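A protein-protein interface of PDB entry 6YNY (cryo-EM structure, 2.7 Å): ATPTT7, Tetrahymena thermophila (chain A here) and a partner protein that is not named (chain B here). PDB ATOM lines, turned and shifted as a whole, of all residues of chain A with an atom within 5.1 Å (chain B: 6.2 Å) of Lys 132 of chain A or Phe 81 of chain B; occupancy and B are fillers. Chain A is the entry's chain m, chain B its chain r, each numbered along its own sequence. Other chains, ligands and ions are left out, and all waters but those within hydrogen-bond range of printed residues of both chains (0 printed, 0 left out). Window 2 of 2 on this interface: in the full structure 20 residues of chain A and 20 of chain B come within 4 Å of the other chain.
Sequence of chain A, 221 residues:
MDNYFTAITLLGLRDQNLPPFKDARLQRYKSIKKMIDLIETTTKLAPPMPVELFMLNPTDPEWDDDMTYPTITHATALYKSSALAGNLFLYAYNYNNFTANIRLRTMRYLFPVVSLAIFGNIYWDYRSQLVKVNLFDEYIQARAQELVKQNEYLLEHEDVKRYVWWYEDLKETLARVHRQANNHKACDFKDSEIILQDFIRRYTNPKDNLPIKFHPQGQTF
O of Tyr 70 of chain B lies within hydrogen-bond range of N of Phe 81 of chain B, at 3.0 Å.
The backbone NH (N) of Gly 79 of chain B is in hydrogen-bond range of the backbone carbonyl oxygen (O) of Ile 71 of chain B (2.9 Å).
The backbone NH (N) of Gly 78 of chain B sits at hydrogen-bond distance from the backbone carbonyl oxygen (O) of Phe 72 of chain B.
Among the printed residues, merely in contact across the chains: Lys 132 of chain A with Phe 81 of chain B (3.3 Å), Val 131 of chain A with Ile 71 of chain B (3.9 Å), Val 131 of chain A with Phe 72 of chain B (3.95 Å) and Leu 135 of chain A with Phe 72 of chain B (3.99 Å).
Lys 132 of chain A touches just one residue of chain B: Phe 81.
Of the printed residues of chain B, Leu 135 of chain A touches Phe 72 (3.99 Å).
Printed residues of chain A within 4 Å of Ile 71 of chain B: Val 131 (3.9 Å).
Gly 78 of chain B touches none of the printed residues of chain A.
Of chain A, only Lys 132 (3.3 Å) comes within 4 Å of Phe 81 of chain B.
The nearest printed residue of chain B that does not touch Leu 135 of chain A is Ile 71 of chain B (4.4 Å).
Of the 10 printed residues of chain B, 3 touch a printed residue of chain A.
Hydrophobic or aromatic side chains of chain B within 4 Å of the printed part of chain A: Ile 71, Phe 72 and Phe 81.
Among the printed residues, 4 pairs touch across the chains.
Among the printed residues, no Asp or Glu carboxylate lies within 4 Å of a Lys or Arg side-chain nitrogen of the other chain.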
ATOM      1  N   PRO A  70     -35.731  10.838  23.184  1.00  0.00           N
ATOM      2  CA  PRO A  70     -34.923   9.716  23.666  1.00  0.00           C
ATOM      3  C   PRO A  70     -35.111   9.505  25.159  1.00  0.00           C
ATOM      4  O   PRO A  70     -35.105  10.453  25.946  1.00  0.00           O
ATOM      5  CB  PRO A  70     -33.491  10.140  23.330  1.00  0.00           C
ATOM      6  CG  PRO A  70     -33.538  11.590  23.236  1.00  0.00           C
ATOM      7  CD  PRO A  70     -34.885  11.946  22.712  1.00  0.00           C
ATOM      8  N   SER A 128     -26.007   3.654  25.719  1.00  0.00           N
ATOM      9  CA  SER A 128     -26.372   4.342  24.487  1.00  0.00           C
ATOM     10  C   SER A 128     -27.541   5.291  24.713  1.00  0.00           C
ATOM     11  O   SER A 128     -27.516   6.443  24.270  1.00  0.00           O
ATOM     12  CB  SER A 128     -26.701   3.324  23.398  1.00  0.00           C
ATOM     13  OG  SER A 128     -27.618   2.360  23.865  1.00  0.00           O
ATOM     14  N   GLN A 129     -28.578   4.825  25.411  1.00  0.00           N
ATOM     15  CA  GLN A 129     -29.701   5.697  25.730  1.00  0.00           C
ATOM     16  C   GLN A 129     -29.240   6.926  26.497  1.00  0.00           C
ATOM     17  O   GLN A 129     -29.731   8.036  26.266  1.00  0.00           O
ATOM     18  CB  GLN A 129     -30.735   4.932  26.546  1.00  0.00           C
ATOM     19  CG  GLN A 129     -31.371   3.775  25.831  1.00  0.00           C
ATOM     20  CD  GLN A 129     -32.008   2.795  26.784  1.00  0.00           C
ATOM     21  OE1 GLN A 129     -32.137   3.062  27.976  1.00  0.00           O
ATOM     22  NE2 GLN A 129     -32.400   1.648  26.267  1.00  0.00           N
ATOM     23  N   LEU A 130     -28.295   6.744  27.417  1.00  0.00           N
ATOM     24  CA  LEU A 130     -27.798   7.857  28.212  1.00  0.00           C
ATOM     25  C   LEU A 130     -27.086   8.885  27.344  1.00  0.00           C
ATOM     26  O   LEU A 130     -27.242  10.094  27.545  1.00  0.00           O
ATOM     27  CB  LEU A 130     -26.869   7.323  29.296  1.00  0.00           C
ATOM     28  CG  LEU A 130     -26.240   8.313  30.264  1.00  0.00           C
ATOM     29  CD1 LEU A 130     -27.303   9.100  30.984  1.00  0.00           C
ATOM     30  CD2 LEU A 130     -25.387   7.555  31.245  1.00  0.00           C
ATOM     31  N   VAL A 131     -26.301   8.422  26.373  1.00  0.00           N
ATOM     32  CA  VAL A 131     -25.589   9.342  25.493  1.00  0.00           C
ATOM     33  C   VAL A 131     -26.571  10.156  24.667  1.00  0.00           C
ATOM     34  O   VAL A 131     -26.424  11.376  24.522  1.00  0.00           O
ATOM     35  CB  VAL A 131     -24.611   8.561  24.599  1.00  0.00           C
ATOM     36  CG1 VAL A 131     -24.002   9.465  23.563  1.00  0.00           C
ATOM     37  CG2 VAL A 131     -23.532   7.926  25.435  1.00  0.00           C
ATOM     38  N   LYS A 132     -27.589   9.500  24.114  1.00  0.00           N
ATOM     39  CA  LYS A 132     -28.549  10.193  23.267  1.00  0.00           C
ATOM     40  C   LYS A 132     -29.332  11.237  24.050  1.00  0.00           C
ATOM     41  O   LYS A 132     -29.565  12.347  23.558  1.00  0.00           O
ATOM     42  CB  LYS A 132     -29.495   9.180  22.633  1.00  0.00           C
ATOM     43  CG  LYS A 132     -28.793   8.122  21.817  1.00  0.00           C
ATOM     44  CD  LYS A 132     -29.763   7.108  21.267  1.00  0.00           C
ATOM     45  CE  LYS A 132     -29.038   5.938  20.656  1.00  0.00           C
ATOM     46  NZ  LYS A 132     -29.974   4.971  20.044  1.00  0.00           N
ATOM     47  N   VAL A 133     -29.751  10.901  25.269  1.00  0.00           N
ATOM     48  CA  VAL A 133     -30.489  11.852  26.092  1.00  0.00           C
ATOM     49  C   VAL A 133     -29.660  13.103  26.331  1.00  0.00           C
ATOM     50  O   VAL A 133     -30.183  14.223  26.331  1.00  0.00           O
ATOM     51  CB  VAL A 133     -30.908  11.191  27.416  1.00  0.00           C
ATOM     52  CG1 VAL A 133     -31.429  12.218  28.389  1.00  0.00           C
ATOM     53  CG2 VAL A 133     -31.953  10.146  27.162  1.00  0.00           C
ATOM     54  N   ASN A 134     -28.355  12.936  26.540  1.00  0.00           N
ATOM     55  CA  ASN A 134     -27.496  14.085  26.791  1.00  0.00           C
ATOM     56  C   ASN A 134     -27.266  14.898  25.524  1.00  0.00           C
ATOM     57  O   ASN A 134     -27.153  16.126  25.592  1.00  0.00           O
ATOM     58  CB  ASN A 134     -26.174  13.620  27.390  1.00  0.00           C
ATOM     59  CG  ASN A 134     -26.341  13.032  28.770  1.00  0.00           C
ATOM     60  OD1 ASN A 134     -27.219  13.439  29.530  1.00  0.00           O
ATOM     61  ND2 ASN A 134     -25.503  12.067  29.104  1.00  0.00           N
ATOM     62  N   LEU A 135     -27.189  14.239  24.369  1.00  0.00           N
ATOM     63  CA  LEU A 135     -27.096  14.967  23.110  1.00  0.00           C
ATOM     64  C   LEU A 135     -28.367  15.760  22.846  1.00  0.00           C
ATOM     65  O   LEU A 135     -28.312  16.903  22.380  1.00  0.00           O
ATOM     66  CB  LEU A 135     -26.832  13.996  21.962  1.00  0.00           C
ATOM     67  CG  LEU A 135     -25.511  13.236  21.984  1.00  0.00           C
ATOM     68  CD1 LEU A 135     -25.482  12.225  20.863  1.00  0.00           C
ATOM     69  CD2 LEU A 135     -24.346  14.184  21.871  1.00  0.00           C
ATOM     70  N   PHE A 136     -29.522  15.164  23.136  1.00  0.00           N
ATOM     71  CA  PHE A 136     -30.793  15.845  22.933  1.00  0.00           C
ATOM     72  C   PHE A 136     -30.923  17.055  23.847  1.00  0.00           C
ATOM     73  O   PHE A 136     -31.403  18.112  23.426  1.00  0.00           O
ATOM     74  CB  PHE A 136     -31.933  14.857  23.169  1.00  0.00           C
ATOM     75  CG  PHE A 136     -33.298  15.442  23.014  1.00  0.00           C
ATOM     76  CD1 PHE A 136     -33.907  15.489  21.779  1.00  0.00           C
ATOM     77  CD2 PHE A 136     -33.984  15.928  24.108  1.00  0.00           C
ATOM     78  CE1 PHE A 136     -35.166  16.019  21.637  1.00  0.00           C
ATOM     79  CE2 PHE A 136     -35.241  16.457  23.969  1.00  0.00           C
ATOM     80  CZ  PHE A 136     -35.833  16.502  22.734  1.00  0.00           C
ATOM     81  N   ASP A 137     -30.490  16.923  25.101  1.00  0.00           N
ATOM     82  CA  ASP A 137     -30.657  18.012  26.056  1.00  0.00           C
ATOM     83  C   ASP A 137     -29.753  19.192  25.721  1.00  0.00           C
ATOM     84  O   ASP A 137     -30.157  20.349  25.874  1.00  0.00           O
ATOM     85  CB  ASP A 137     -30.383  17.516  27.473  1.00  0.00           C
ATOM     86  CG  ASP A 137     -31.468  16.592  27.991  1.00  0.00           C
ATOM     87  OD1 ASP A 137     -32.629  16.721  27.547  1.00  0.00           O
ATOM     88  OD2 ASP A 137     -31.164  15.741  28.853  1.00  0.00           O
ATOM     89  N   TYR B  70     -19.662   3.808  18.232  1.00  0.00           N
ATOM     90  CA  TYR B  70     -20.850   3.438  17.475  1.00  0.00           C
ATOM     91  C   TYR B  70     -21.697   4.650  17.125  1.00  0.00           C
ATOM     92  O   TYR B  70     -22.320   4.681  16.060  1.00  0.00           O
ATOM     93  CB  TYR B  70     -21.663   2.434  18.288  1.00  0.00           C
ATOM     94  CG  TYR B  70     -22.982   2.019  17.690  1.00  0.00           C
ATOM     95  CD1 TYR B  70     -23.036   1.127  16.634  1.00  0.00           C
ATOM     96  CD2 TYR B  70     -24.175   2.495  18.204  1.00  0.00           C
ATOM     97  CE1 TYR B  70     -24.238   0.740  16.096  1.00  0.00           C
ATOM     98  CE2 TYR B  70     -25.378   2.111  17.672  1.00  0.00           C
ATOM     99  CZ  TYR B  70     -25.406   1.232  16.620  1.00  0.00           C
ATOM    100  OH  TYR B  70     -26.612   0.849  16.089  1.00  0.00           O
ATOM    101  N   ILE B  71     -21.729   5.646  18.002  1.00  0.00           N
ATOM    102  CA  ILE B  71     -22.580   6.813  17.814  1.00  0.00           C
ATOM    103  C   ILE B  71     -21.836   7.936  17.107  1.00  0.00           C
ATOM    104  O   ILE B  71     -22.302   8.462  16.094  1.00  0.00           O
ATOM    105  CB  ILE B  71     -23.128   7.275  19.179  1.00  0.00           C
ATOM    106  CG1 ILE B  71     -23.995   6.177  19.792  1.00  0.00           C
ATOM    107  CG2 ILE B  71     -23.911   8.552  19.028  1.00  0.00           C
ATOM    108  CD1 ILE B  71     -24.413   6.443  21.197  1.00  0.00           C
ATOM    109  N   PHE B  72     -20.671   8.318  17.623  1.00  0.00           N
ATOM    110  CA  PHE B  72     -19.930   9.446  17.080  1.00  0.00           C
ATOM    111  C   PHE B  72     -19.047   9.054  15.905  1.00  0.00           C
ATOM    112  O   PHE B  72     -18.950   9.801  14.928  1.00  0.00           O
ATOM    113  CB  PHE B  72     -19.073  10.078  18.173  1.00  0.00           C
ATOM    114  CG  PHE B  72     -19.858  10.585  19.337  1.00  0.00           C
ATOM    115  CD1 PHE B  72     -20.459  11.823  19.296  1.00  0.00           C
ATOM    116  CD2 PHE B  72     -19.986   9.825  20.480  1.00  0.00           C
ATOM    117  CE1 PHE B  72     -21.178  12.289  20.367  1.00  0.00           C
ATOM    118  CE2 PHE B  72     -20.702  10.288  21.552  1.00  0.00           C
ATOM    119  CZ  PHE B  72     -21.299  11.522  21.496  1.00  0.00           C
ATOM    120  N   GLY B  78     -20.441  10.840  13.216  1.00  0.00           N
ATOM    121  CA  GLY B  78     -21.448   9.804  13.199  1.00  0.00           C
ATOM    122  C   GLY B  78     -20.882   8.460  12.804  1.00  0.00           C
ATOM    123  O   GLY B  78     -20.100   8.354  11.856  1.00  0.00           O
ATOM    124  N   GLY B  79     -21.271   7.424  13.538  1.00  0.00           N
ATOM    125  CA  GLY B  79     -20.816   6.076  13.277  1.00  0.00           C
ATOM    126  C   GLY B  79     -21.871   5.198  12.645  1.00  0.00           C
ATOM    127  O   GLY B  79     -22.793   5.689  11.988  1.00  0.00           O
ATOM    128  N   LYS B  80     -21.745   3.886  12.845  1.00  0.00           N
ATOM    129  CA  LYS B  80     -22.697   2.938  12.288  1.00  0.00           C
ATOM    130  C   LYS B  80     -24.104   3.139  12.827  1.00  0.00           C
ATOM    131  O   LYS B  80     -25.051   2.584  12.262  1.00  0.00           O
ATOM    132  CB  LYS B  80     -22.230   1.515  12.573  1.00  0.00           C
ATOM    133  CG  LYS B  80     -20.943   1.147  11.872  1.00  0.00           C
ATOM    134  CD  LYS B  80     -20.536  -0.283  12.167  1.00  0.00           C
ATOM    135  CE  LYS B  80     -19.215  -0.625  11.502  1.00  0.00           C
ATOM    136  NZ  LYS B  80     -18.746  -1.994  11.831  1.00  0.00           N
ATOM    137  N   PHE B  81     -24.263   3.919  13.896  1.00  0.00           N
ATOM    138  CA  PHE B  81     -25.594   4.221  14.405  1.00  0.00           C
ATOM    139  C   PHE B  81     -26.460   4.886  13.346  1.00  0.00           C
ATOM    140  O   PHE B  81     -27.687   4.747  13.371  1.00  0.00           O
ATOM    141  CB  PHE B  81     -25.477   5.110  15.641  1.00  0.00           C
ATOM    142  CG  PHE B  81     -26.764   5.740  16.062  1.00  0.00           C
ATOM    143  CD1 PHE B  81     -26.944   7.101  15.947  1.00  0.00           C
ATOM    144  CD2 PHE B  81     -27.793   4.976  16.572  1.00  0.00           C
ATOM    145  CE1 PHE B  81     -28.119   7.687  16.332  1.00  0.00           C
ATOM    146  CE2 PHE B  81     -28.973   5.559  16.959  1.00  0.00           C
ATOM    147  CZ  PHE B  81     -29.137   6.916  16.839  1.00  0.00           C
ATOM    148  N   LEU B  82     -25.847   5.603  12.411  1.00  0.00           N
ATOM    149  CA  LEU B  82     -26.576   6.271  11.345  1.00  0.00           C
ATOM    150  C   LEU B  82     -26.855   5.361  10.157  1.00  0.00           C
ATOM    151  O   LEU B  82     -27.527   5.788   9.214  1.00  0.00           O
ATOM    152  CB  LEU B  82     -25.800   7.499  10.873  1.00  0.00           C
ATOM    153  CG  LEU B  82     -25.579   8.598  11.907  1.00  0.00           C
ATOM    154  CD1 LEU B  82     -24.821   9.752  11.289  1.00  0.00           C
ATOM    155  CD2 LEU B  82     -26.894   9.072  12.478  1.00  0.00           C
ATOM    156  N   GLU B  83     -26.362   4.129  10.180  1.00  0.00           N
ATOM    157  CA  GLU B  83     -26.568   3.208   9.076  1.00  0.00           C
ATOM    158  C   GLU B  83     -27.907   2.500   9.212  1.00  0.00           C
ATOM    159  O   GLU B  83     -28.303   2.089  10.305  1.00  0.00           O
ATOM    160  CB  GLU B  83     -25.444   2.177   9.020  1.00  0.00           C
ATOM    161  CG  GLU B  83     -24.100   2.749   8.645  1.00  0.00           C
ATOM    162  CD  GLU B  83     -23.016   1.693   8.586  1.00  0.00           C
ATOM    163  OE1 GLU B  83     -23.324   0.510   8.839  1.00  0.00           O
ATOM    164  OE2 GLU B  83     -21.856   2.044   8.287  1.00  0.00           O
ATOM    165  N   MET B  84     -28.608   2.369   8.091  1.00  0.00           N
ATOM    166  CA  MET B  84     -29.853   1.620   8.044  1.00  0.00           C
ATOM    167  C   MET B  84     -29.945   0.920   6.701  1.00  0.00           C
ATOM    168  O   MET B  84     -29.676   1.527   5.661  1.00  0.00           O
ATOM    169  CB  MET B  84     -31.064   2.530   8.265  1.00  0.00           C
ATOM    170  CG  MET B  84     -31.196   3.655   7.283  1.00  0.00           C
ATOM    171  SD  MET B  84     -32.526   4.777   7.739  1.00  0.00           S
ATOM    172  CE  MET B  84     -32.341   6.027   6.487  1.00  0.00           C
